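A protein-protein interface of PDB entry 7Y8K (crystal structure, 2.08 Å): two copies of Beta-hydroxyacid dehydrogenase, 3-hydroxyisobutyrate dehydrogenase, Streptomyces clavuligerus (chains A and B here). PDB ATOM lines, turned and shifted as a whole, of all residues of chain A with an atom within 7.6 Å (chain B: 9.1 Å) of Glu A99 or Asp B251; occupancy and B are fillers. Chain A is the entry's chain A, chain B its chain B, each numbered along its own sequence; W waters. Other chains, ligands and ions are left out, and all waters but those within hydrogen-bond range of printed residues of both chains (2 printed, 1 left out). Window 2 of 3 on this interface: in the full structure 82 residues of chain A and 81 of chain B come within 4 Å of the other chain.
The side-chain hydroxyl (OG1) of Thr A97 sits at hydrogen-bond distance from the backbone NH (N) of Lys A100 (2.9 Å).
The backbone carbonyl oxygen (O) of Thr A97 is in hydrogen-bond range of the side-chain hydroxyl (OG1) of Thr A101, 2.8 Å away.
The side-chain amide nitrogen (ND2) of Asn B194 is in hydrogen-bond range of the side-chain hydroxyl (OG) of Ser B252 (2.9 Å).
A ring nitrogen (ND1) of His B247 sits at hydrogen-bond distance from the backbone carbonyl oxygen (O) of Glu B243.
The backbone carbonyl oxygen of His B244 sits at hydrogen-bond distance from the side-chain hydroxyl of Thr B248 (2.8 Å).
O of Thr B248 sits at hydrogen-bond distance from OG of Ser B252.
Among the printed residues, pairs that only touch across the chains: Asp A96 with His B244 (3.6 Å), Thr A97 with His B244 (3.8 Å), Thr A97 with His B247 (3.7 Å), Thr A97 with Thr B248 (3.4 Å), Thr A97 with Asp B251 (3.6 Å), Pro A98 with Thr B248 (3.4 Å), Glu A99 with Asp B251 (3.95 Å), Leu A168 with Leu B190 (3.96 Å), Leu A168 with Asn B194 (3.5 Å), Lys A288 with Ala B193 (3.9 Å), Lys A288 with Ser B252 (3.4 Å) and Lys A288 with Gly B253 (3.4 Å).
Tyr A71 touches none of the printed residues of chain B.
Glu A99 touches just one residue of chain B: Asp B251.
Of the printed residues of chain B, Leu A168 touches Leu B190 and Asn B194.
Of the printed residues of chain A, Ala B193 touches Lys A288 (3.9 Å).
Of the printed residues of chain A, Thr B248 touches Thr A97 (3.4 Å) and Pro A98 (3.4 Å).
No residue of chain A comes within 4 Å of Ala B250.
Of chain A, only Thr A97 and Glu A99 come within 4 Å of Asp B251.
Printed residues of chain A within 4 Å of Gly B253: Lys A288 (3.4 Å).
The nearest printed residue of chain A that does not touch His B244 is Tyr A71 (5.8 Å).
Of the 17 printed residues of chain A, 6 touch a printed residue of chain B.
Hydrophobic or aromatic side chains of chain A that line the printed part of chain B: Pro A98 and Leu A168.
Hydrophobic or aromatic side chains of chain B that line the printed part of chain A: Leu B190, Ala B193, His B244 and His B247.
Among the printed residues, 12 pairs touch across the chains.
No position is printed for both chains.
Of the 12 pairs that touch across the chains among the printed residues, none has its exchanged pair printed and touching as well.
Water W2 lies within hydrogen-bond range of OD2 of Asp B251 (2.9 Å), N of Glu A99 (3.1 Å) and OG1 of Thr A97 (3.4 Å).
Water W1 bridges N of Lys A288 (3.2 Å) and N of Ala B193 (3.3 Å).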
ATOM      1  N   TYR A  71      23.851 -16.379  -0.234  1.00  0.00           N
ATOM      2  CA  TYR A  71      23.705 -16.193   1.207  1.00  0.00           C
ATOM      3  C   TYR A  71      24.150 -17.424   1.990  1.00  0.00           C
ATOM      4  O   TYR A  71      24.569 -17.286   3.142  1.00  0.00           O
ATOM      5  CB  TYR A  71      22.262 -15.809   1.573  1.00  0.00           C
ATOM      6  CG  TYR A  71      22.043 -14.293   1.629  1.00  0.00           C
ATOM      7  CD1 TYR A  71      22.284 -13.507   0.519  1.00  0.00           C
ATOM      8  CD2 TYR A  71      21.592 -13.654   2.795  1.00  0.00           C
ATOM      9  CE1 TYR A  71      22.088 -12.148   0.551  1.00  0.00           C
ATOM     10  CE2 TYR A  71      21.409 -12.276   2.840  1.00  0.00           C
ATOM     11  CZ  TYR A  71      21.659 -11.530   1.707  1.00  0.00           C
ATOM     12  OH  TYR A  71      21.469 -10.154   1.687  1.00  0.00           O
ATOM     13  N   TYR A  75      26.558 -17.845   5.717  1.00  0.00           N
ATOM     14  CA  TYR A  75      26.431 -18.769   6.848  1.00  0.00           C
ATOM     15  C   TYR A  75      27.722 -19.549   7.067  1.00  0.00           C
ATOM     16  O   TYR A  75      28.126 -19.789   8.212  1.00  0.00           O
ATOM     17  CB  TYR A  75      25.282 -19.747   6.619  1.00  0.00           C
ATOM     18  CG  TYR A  75      23.890 -19.150   6.521  1.00  0.00           C
ATOM     19  CD1 TYR A  75      23.399 -18.314   7.510  1.00  0.00           C
ATOM     20  CD2 TYR A  75      23.040 -19.490   5.473  1.00  0.00           C
ATOM     21  CE1 TYR A  75      22.105 -17.787   7.441  1.00  0.00           C
ATOM     22  CE2 TYR A  75      21.732 -18.973   5.393  1.00  0.00           C
ATOM     23  CZ  TYR A  75      21.274 -18.115   6.383  1.00  0.00           C
ATOM     24  OH  TYR A  75      19.996 -17.586   6.317  1.00  0.00           O
ATOM     25  N   ASP A  96      20.971 -13.513  -4.338  1.00  0.00           N
ATOM     26  CA  ASP A  96      20.214 -14.668  -3.852  1.00  0.00           C
ATOM     27  C   ASP A  96      18.728 -14.352  -4.009  1.00  0.00           C
ATOM     28  O   ASP A  96      18.352 -13.227  -4.342  1.00  0.00           O
ATOM     29  CB  ASP A  96      20.553 -15.008  -2.397  1.00  0.00           C
ATOM     30  CG  ASP A  96      20.589 -16.505  -2.144  1.00  0.00           C
ATOM     31  OD1 ASP A  96      19.618 -17.173  -2.518  1.00  0.00           O
ATOM     32  OD2 ASP A  96      21.598 -17.019  -1.602  1.00  0.00           O
ATOM     33  N   THR A  97      17.883 -15.352  -3.760  1.00  0.00           N
ATOM     34  CA  THR A  97      16.443 -15.120  -3.822  1.00  0.00           C
ATOM     35  C   THR A  97      15.995 -14.175  -2.710  1.00  0.00           C
ATOM     36  O   THR A  97      16.671 -14.040  -1.685  1.00  0.00           O
ATOM     37  CB  THR A  97      15.658 -16.423  -3.706  1.00  0.00           C
ATOM     38  OG1 THR A  97      15.483 -16.749  -2.318  1.00  0.00           O
ATOM     39  CG2 THR A  97      16.374 -17.549  -4.437  1.00  0.00           C
ATOM     40  N   PRO A  98      14.851 -13.497  -2.906  1.00  0.00           N
ATOM     41  CA  PRO A  98      14.302 -12.673  -1.820  1.00  0.00           C
ATOM     42  C   PRO A  98      14.014 -13.460  -0.559  1.00  0.00           C
ATOM     43  O   PRO A  98      14.188 -12.931   0.548  1.00  0.00           O
ATOM     44  CB  PRO A  98      13.024 -12.092  -2.446  1.00  0.00           C
ATOM     45  CG  PRO A  98      13.341 -12.013  -3.905  1.00  0.00           C
ATOM     46  CD  PRO A  98      14.121 -13.293  -4.166  1.00  0.00           C
ATOM     47  N   GLU A  99      13.587 -14.720  -0.687  1.00  0.00           N
ATOM     48  CA  GLU A  99      13.286 -15.508   0.505  1.00  0.00           C
ATOM     49  C   GLU A  99      14.559 -15.866   1.265  1.00  0.00           C
ATOM     50  O   GLU A  99      14.592 -15.783   2.499  1.00  0.00           O
ATOM     51  CB  GLU A  99      12.501 -16.767   0.128  1.00  0.00           C
ATOM     52  CG  GLU A  99      12.096 -17.632   1.323  1.00  0.00           C
ATOM     53  CD  GLU A  99      11.103 -16.933   2.243  1.00  0.00           C
ATOM     54  OE1 GLU A  99      10.371 -16.023   1.787  1.00  0.00           O
ATOM     55  OE2 GLU A  99      11.034 -17.307   3.429  1.00  0.00           O
ATOM     56  N   LYS A 100      15.617 -16.274   0.555  1.00  0.00           N
ATOM     57  CA  LYS A 100      16.877 -16.561   1.250  1.00  0.00           C
ATOM     58  C   LYS A 100      17.482 -15.300   1.869  1.00  0.00           C
ATOM     59  O   LYS A 100      18.096 -15.370   2.941  1.00  0.00           O
ATOM     60  CB  LYS A 100      17.884 -17.218   0.305  1.00  0.00           C
ATOM     61  CG  LYS A 100      17.531 -18.633  -0.091  1.00  0.00           C
ATOM     62  CD  LYS A 100      17.899 -19.626   1.007  1.00  0.00           C
ATOM     63  CE  LYS A 100      19.335 -20.110   0.877  1.00  0.00           C
ATOM     64  NZ  LYS A 100      20.014 -20.190   2.190  1.00  0.00           N
ATOM     65  N   THR A 101      17.316 -14.150   1.212  1.00  0.00           N
ATOM     66  CA  THR A 101      17.782 -12.881   1.770  1.00  0.00           C
ATOM     67  C   THR A 101      17.031 -12.522   3.045  1.00  0.00           C
ATOM     68  O   THR A 101      17.606 -11.956   3.986  1.00  0.00           O
ATOM     69  CB  THR A 101      17.595 -11.772   0.733  1.00  0.00           C
ATOM     70  OG1 THR A 101      18.262 -12.131  -0.484  1.00  0.00           O
ATOM     71  CG2 THR A 101      18.122 -10.449   1.250  1.00  0.00           C
ATOM     72  N   ARG A 102      15.722 -12.796   3.070  1.00  0.00           N
ATOM     73  CA  ARG A 102      14.912 -12.535   4.255  1.00  0.00           C
ATOM     74  C   ARG A 102      15.310 -13.448   5.404  1.00  0.00           C
ATOM     75  O   ARG A 102      15.287 -13.037   6.568  1.00  0.00           O
ATOM     76  CB  ARG A 102      13.425 -12.711   3.922  1.00  0.00           C
ATOM     77  CG  ARG A 102      12.834 -11.549   3.172  1.00  0.00           C
ATOM     78  CD  ARG A 102      11.471 -11.889   2.591  1.00  0.00           C
ATOM     79  NE  ARG A 102      11.030 -10.841   1.676  1.00  0.00           N
ATOM     80  CZ  ARG A 102      10.549 -11.060   0.461  1.00  0.00           C
ATOM     81  NH1 ARG A 102      10.422 -12.284  -0.019  1.00  0.00           N
ATOM     82  NH2 ARG A 102      10.172 -10.024  -0.284  1.00  0.00           N
ATOM     83  N   ALA A 103      15.658 -14.698   5.097  1.00  0.00           N
ATOM     84  CA  ALA A 103      16.130 -15.615   6.131  1.00  0.00           C
ATOM     85  C   ALA A 103      17.518 -15.218   6.637  1.00  0.00           C
ATOM     86  O   ALA A 103      17.770 -15.221   7.849  1.00  0.00           O
ATOM     87  CB  ALA A 103      16.130 -17.051   5.593  1.00  0.00           C
ATOM     88  N   GLY A 104      18.437 -14.892   5.723  1.00  0.00           N
ATOM     89  CA  GLY A 104      19.720 -14.351   6.145  1.00  0.00           C
ATOM     90  C   GLY A 104      19.562 -13.147   7.054  1.00  0.00           C
ATOM     91  O   GLY A 104      20.257 -13.032   8.062  1.00  0.00           O
ATOM     92  N   ALA A 105      18.613 -12.257   6.722  1.00  0.00           N
ATOM     93  CA  ALA A 105      18.304 -11.090   7.550  1.00  0.00           C
ATOM     94  C   ALA A 105      17.814 -11.481   8.941  1.00  0.00           C
ATOM     95  O   ALA A 105      18.185 -10.845   9.935  1.00  0.00           O
ATOM     96  CB  ALA A 105      17.253 -10.226   6.852  1.00  0.00           C
ATOM     97  N   PRO A 163      13.847  -6.762   3.489  1.00  0.00           N
ATOM     98  CA  PRO A 163      15.173  -7.173   3.022  1.00  0.00           C
ATOM     99  C   PRO A 163      15.128  -7.849   1.636  1.00  0.00           C
ATOM    100  O   PRO A 163      16.080  -7.757   0.942  1.00  0.00           O
ATOM    101  CB  PRO A 163      15.646  -8.133   4.108  1.00  0.00           C
ATOM    102  CG  PRO A 163      14.862  -7.726   5.322  1.00  0.00           C
ATOM    103  CD  PRO A 163      13.503  -7.374   4.769  1.00  0.00           C
ATOM    104  N   GLY A 164      13.994  -8.423   1.252  1.00  0.00           N
ATOM    105  CA  GLY A 164      13.855  -9.092  -0.050  1.00  0.00           C
ATOM    106  C   GLY A 164      13.687  -8.155  -1.233  1.00  0.00           C
ATOM    107  O   GLY A 164      13.933  -8.616  -2.326  1.00  0.00           O
ATOM    108  N   ALA A 167      16.716  -7.722  -3.346  1.00  0.00           N
ATOM    109  CA  ALA A 167      16.948  -8.986  -4.031  1.00  0.00           C
ATOM    110  C   ALA A 167      15.953  -9.183  -5.175  1.00  0.00           C
ATOM    111  O   ALA A 167      16.342  -9.551  -6.294  1.00  0.00           O
ATOM    112  CB  ALA A 167      16.867 -10.125  -3.012  1.00  0.00           C
ATOM    113  N   LEU A 168      14.663  -8.913  -4.928  1.00  0.00           N
ATOM    114  CA  LEU A 168      13.665  -9.098  -5.981  1.00  0.00           C
ATOM    115  C   LEU A 168      13.995  -8.247  -7.199  1.00  0.00           C
ATOM    116  O   LEU A 168      13.978  -8.739  -8.334  1.00  0.00           O
ATOM    117  CB  LEU A 168      12.260  -8.761  -5.465  1.00  0.00           C
ATOM    118  CG  LEU A 168      11.126  -9.000  -6.485  1.00  0.00           C
ATOM    119  CD1 LEU A 168      10.786 -10.500  -6.591  1.00  0.00           C
ATOM    120  CD2 LEU A 168       9.897  -8.204  -6.136  1.00  0.00           C
ATOM    121  N   LYS A 288       1.355 -16.547 -11.656  1.00  0.00           N
ATOM    122  CA  LYS A 288       0.935 -17.536 -10.626  1.00  0.00           C
ATOM    123  C   LYS A 288      -0.542 -17.923 -10.826  1.00  0.00           C
ATOM    124  O   LYS A 288      -0.819 -19.116 -10.933  1.00  0.00           O
ATOM    125  CB  LYS A 288       1.228 -16.999  -9.218  1.00  0.00           C
ATOM    126  CG  LYS A 288       0.628 -15.650  -8.862  1.00  0.00           C
ATOM    127  CD  LYS A 288       1.202 -15.072  -7.590  1.00  0.00           C
ATOM    128  CE  LYS A 288       1.556 -16.115  -6.551  1.00  0.00           C
ATOM    129  NZ  LYS A 288       0.351 -16.695  -5.915  1.00  0.00           N
ATOM    130  N   LEU B 190       7.276 -12.090 -12.550  1.00  0.00           N
ATOM    131  CA  LEU B 190       7.876 -12.046 -11.191  1.00  0.00           C
ATOM    132  C   LEU B 190       7.375 -10.797 -10.467  1.00  0.00           C
ATOM    133  O   LEU B 190       7.005 -10.907  -9.302  1.00  0.00           O
ATOM    134  CB  LEU B 190       9.394 -12.024 -11.368  1.00  0.00           C
ATOM    135  CG  LEU B 190      10.265 -12.203 -10.133  1.00  0.00           C
ATOM    136  CD1 LEU B 190       9.732 -13.313  -9.257  1.00  0.00           C
ATOM    137  CD2 LEU B 190      11.691 -12.511 -10.557  1.00  0.00           C
ATOM    138  N   ALA B 193       3.722 -11.241  -9.546  1.00  0.00           N
ATOM    139  CA  ALA B 193       3.661 -12.180  -8.434  1.00  0.00           C
ATOM    140  C   ALA B 193       3.999 -11.533  -7.107  1.00  0.00           C
ATOM    141  O   ALA B 193       3.564 -12.023  -6.061  1.00  0.00           O
ATOM    142  CB  ALA B 193       4.622 -13.341  -8.678  1.00  0.00           C
ATOM    143  N   ASN B 194       4.757 -10.444  -7.117  1.00  0.00           N
ATOM    144  CA  ASN B 194       5.127  -9.763  -5.889  1.00  0.00           C
ATOM    145  C   ASN B 194       4.458  -8.408  -5.751  1.00  0.00           C
ATOM    146  O   ASN B 194       4.973  -7.540  -5.045  1.00  0.00           O
ATOM    147  CB  ASN B 194       6.641  -9.624  -5.811  1.00  0.00           C
ATOM    148  CG  ASN B 194       7.295 -10.918  -5.482  1.00  0.00           C
ATOM    149  OD1 ASN B 194       7.568 -11.200  -4.318  1.00  0.00           O
ATOM    150  ND2 ASN B 194       7.524 -11.743  -6.498  1.00  0.00           N
ATOM    151  N   GLU B 243      20.512 -19.666 -11.376  1.00  0.00           N
ATOM    152  CA  GLU B 243      19.893 -20.519 -10.361  1.00  0.00           C
ATOM    153  C   GLU B 243      19.067 -19.702  -9.371  1.00  0.00           C
ATOM    154  O   GLU B 243      17.967 -20.113  -8.968  1.00  0.00           O
ATOM    155  CB  GLU B 243      20.986 -21.312  -9.627  1.00  0.00           C
ATOM    156  CG  GLU B 243      21.353 -22.601 -10.306  1.00  0.00           C
ATOM    157  CD  GLU B 243      22.701 -23.162  -9.867  1.00  0.00           C
ATOM    158  OE1 GLU B 243      23.230 -22.766  -8.794  1.00  0.00           O
ATOM    159  OE2 GLU B 243      23.229 -24.015 -10.611  1.00  0.00           O
ATOM    160  N   HIS B 244      19.583 -18.538  -8.961  1.00  0.00           N
ATOM    161  CA  HIS B 244      18.801 -17.672  -8.090  1.00  0.00           C
ATOM    162  C   HIS B 244      17.543 -17.177  -8.797  1.00  0.00           C
ATOM    163  O   HIS B 244      16.460 -17.157  -8.196  1.00  0.00           O
ATOM    164  CB  HIS B 244      19.656 -16.502  -7.603  1.00  0.00           C
ATOM    165  CG  HIS B 244      20.858 -16.930  -6.819  1.00  0.00           C
ATOM    166  ND1 HIS B 244      21.959 -16.123  -6.642  1.00  0.00           N
ATOM    167  CD2 HIS B 244      21.139 -18.094  -6.184  1.00  0.00           C
ATOM    168  CE1 HIS B 244      22.864 -16.763  -5.927  1.00  0.00           C
ATOM    169  NE2 HIS B 244      22.395 -17.963  -5.639  1.00  0.00           N
ATOM    170  N   ILE B 245      17.663 -16.779 -10.072  1.00  0.00           N
ATOM    171  CA  ILE B 245      16.478 -16.360 -10.836  1.00  0.00           C
ATOM    172  C   ILE B 245      15.448 -17.483 -10.864  1.00  0.00           C
ATOM    173  O   ILE B 245      14.275 -17.292 -10.520  1.00  0.00           O
ATOM    174  CB  ILE B 245      16.864 -15.935 -12.267  1.00  0.00           C
ATOM    175  CG1 ILE B 245      17.549 -14.563 -12.274  1.00  0.00           C
ATOM    176  CG2 ILE B 245      15.621 -15.941 -13.188  1.00  0.00           C
ATOM    177  CD1 ILE B 245      18.693 -14.456 -13.330  1.00  0.00           C
ATOM    178  N   LEU B 246      15.882 -18.671 -11.272  1.00  0.00           N
ATOM    179  CA  LEU B 246      15.015 -19.843 -11.288  1.00  0.00           C
ATOM    180  C   LEU B 246      14.271 -19.998  -9.968  1.00  0.00           C
ATOM    181  O   LEU B 246      13.038 -20.120  -9.941  1.00  0.00           O
ATOM    182  CB  LEU B 246      15.863 -21.079 -11.603  1.00  0.00           C
ATOM    183  CG  LEU B 246      15.250 -22.479 -11.511  1.00  0.00           C
ATOM    184  CD1 LEU B 246      14.158 -22.640 -12.553  1.00  0.00           C
ATOM    185  CD2 LEU B 246      16.329 -23.575 -11.673  1.00  0.00           C
ATOM    186  N   HIS B 247      14.999 -19.953  -8.854  1.00  0.00           N
ATOM    187  CA  HIS B 247      14.366 -20.202  -7.562  1.00  0.00           C
ATOM    188  C   HIS B 247      13.504 -19.033  -7.109  1.00  0.00           C
ATOM    189  O   HIS B 247      12.471 -19.246  -6.467  1.00  0.00           O
ATOM    190  CB  HIS B 247      15.426 -20.524  -6.513  1.00  0.00           C
ATOM    191  CG  HIS B 247      15.904 -21.929  -6.590  1.00  0.00           C
ATOM    192  ND1 HIS B 247      16.835 -22.339  -7.520  1.00  0.00           N
ATOM    193  CD2 HIS B 247      15.552 -23.033  -5.889  1.00  0.00           C
ATOM    194  CE1 HIS B 247      17.060 -23.633  -7.368  1.00  0.00           C
ATOM    195  NE2 HIS B 247      16.295 -24.079  -6.386  1.00  0.00           N
ATOM    196  N   THR B 248      13.913 -17.804  -7.428  1.00  0.00           N
ATOM    197  CA  THR B 248      13.068 -16.644  -7.167  1.00  0.00           C
ATOM    198  C   THR B 248      11.708 -16.771  -7.858  1.00  0.00           C
ATOM    199  O   THR B 248      10.667 -16.469  -7.259  1.00  0.00           O
ATOM    200  CB  THR B 248      13.789 -15.376  -7.627  1.00  0.00           C
ATOM    201  OG1 THR B 248      15.001 -15.220  -6.878  1.00  0.00           O
ATOM    202  CG2 THR B 248      12.913 -14.147  -7.438  1.00  0.00           C
ATOM    203  N   MET B 249      11.701 -17.197  -9.131  1.00  0.00           N
ATOM    204  CA  MET B 249      10.445 -17.351  -9.860  1.00  0.00           C
ATOM    205  C   MET B 249       9.639 -18.553  -9.375  1.00  0.00           C
ATOM    206  O   MET B 249       8.406 -18.477  -9.286  1.00  0.00           O
ATOM    207  CB  MET B 249      10.688 -17.451 -11.371  1.00  0.00           C
ATOM    208  CG  MET B 249      11.445 -16.273 -11.944  1.00  0.00           C
ATOM    209  SD  MET B 249      11.879 -16.487 -13.682  1.00  0.00           S
ATOM    210  CE  MET B 249      10.304 -16.946 -14.399  1.00  0.00           C
ATOM    211  N   ALA B 250      10.297 -19.668  -9.075  1.00  0.00           N
ATOM    212  CA  ALA B 250       9.581 -20.757  -8.419  1.00  0.00           C
ATOM    213  C   ALA B 250       9.011 -20.296  -7.083  1.00  0.00           C
ATOM    214  O   ALA B 250       7.838 -20.545  -6.776  1.00  0.00           O
ATOM    215  CB  ALA B 250      10.493 -21.964  -8.231  1.00  0.00           C
ATOM    216  N   ASP B 251       9.830 -19.599  -6.284  1.00  0.00           N
ATOM    217  CA  ASP B 251       9.370 -19.059  -5.008  1.00  0.00           C
ATOM    218  C   ASP B 251       8.187 -18.116  -5.168  1.00  0.00           C
ATOM    219  O   ASP B 251       7.440 -17.915  -4.203  1.00  0.00           O
ATOM    220  CB  ASP B 251      10.499 -18.307  -4.290  1.00  0.00           C
ATOM    221  CG  ASP B 251      11.496 -19.231  -3.617  1.00  0.00           C
ATOM    222  OD1 ASP B 251      11.172 -20.409  -3.402  1.00  0.00           O
ATOM    223  OD2 ASP B 251      12.602 -18.769  -3.279  1.00  0.00           O
ATOM    224  N   SER B 252       8.011 -17.518  -6.348  1.00  0.00           N
ATOM    225  CA  SER B 252       6.913 -16.594  -6.605  1.00  0.00           C
ATOM    226  C   SER B 252       5.731 -17.249  -7.302  1.00  0.00           C
ATOM    227  O   SER B 252       4.759 -16.555  -7.607  1.00  0.00           O
ATOM    228  CB  SER B 252       7.402 -15.402  -7.446  1.00  0.00           C
ATOM    229  OG  SER B 252       8.213 -14.519  -6.673  1.00  0.00           O
ATOM    230  N   GLY B 253       5.797 -18.551  -7.579  1.00  0.00           N
ATOM    231  CA  GLY B 253       4.730 -19.234  -8.286  1.00  0.00           C
ATOM    232  C   GLY B 253       4.707 -19.040  -9.785  1.00  0.00           C
ATOM    233  O   GLY B 253       3.746 -19.468 -10.437  1.00  0.00           O
ATOM    234  N   VAL B 254       5.737 -18.434 -10.352  1.00  0.00           N
ATOM    235  CA  VAL B 254       5.808 -18.163 -11.781  1.00  0.00           C
ATOM    236  C   VAL B 254       6.313 -19.395 -12.522  1.00  0.00           C
ATOM    237  O   VAL B 254       7.129 -20.159 -11.997  1.00  0.00           O
ATOM    238  CB  VAL B 254       6.724 -16.946 -11.988  1.00  0.00           C
ATOM    239  CG1 VAL B 254       6.965 -16.670 -13.457  1.00  0.00           C
ATOM    240  CG2 VAL B 254       6.147 -15.758 -11.234  1.00  0.00           C
ATOM    241  N   ASP B 255       5.818 -19.609 -13.745  1.00  0.00           N
ATOM    242  CA  ASP B 255       6.282 -20.747 -14.533  1.00  0.00           C
ATOM    243  C   ASP B 255       7.789 -20.667 -14.737  1.00  0.00           C
ATOM    244  O   ASP B 255       8.334 -19.586 -14.974  1.00  0.00           O
ATOM    245  CB  ASP B 255       5.580 -20.814 -15.896  1.00  0.00           C
ATOM    246  CG  ASP B 255       5.747 -22.177 -16.559  1.00  0.00           C
ATOM    247  OD1 ASP B 255       5.041 -23.127 -16.151  1.00  0.00           O
ATOM    248  OD2 ASP B 255       6.602 -22.321 -17.466  1.00  0.00           O
ATOM    249  N   THR B 256       8.464 -21.821 -14.654  1.00  0.00           N
ATOM    250  CA  THR B 256       9.929 -21.863 -14.656  1.00  0.00           C
ATOM    251  C   THR B 256      10.537 -22.690 -15.790  1.00  0.00           C
ATOM    252  O   THR B 256      11.740 -22.963 -15.748  1.00  0.00           O
ATOM    253  CB  THR B 256      10.470 -22.404 -13.326  1.00  0.00           C
ATOM    254  OG1 THR B 256       9.915 -23.698 -13.067  1.00  0.00           O
ATOM    255  CG2 THR B 256      10.124 -21.469 -12.182  1.00  0.00           C
HETATM  256  O   HOH W   1       2.611 -13.661 -11.419  1.00  0.00           O
HETATM  257  O   HOH W   2      12.333 -15.932  -3.234  1.00  0.00           O
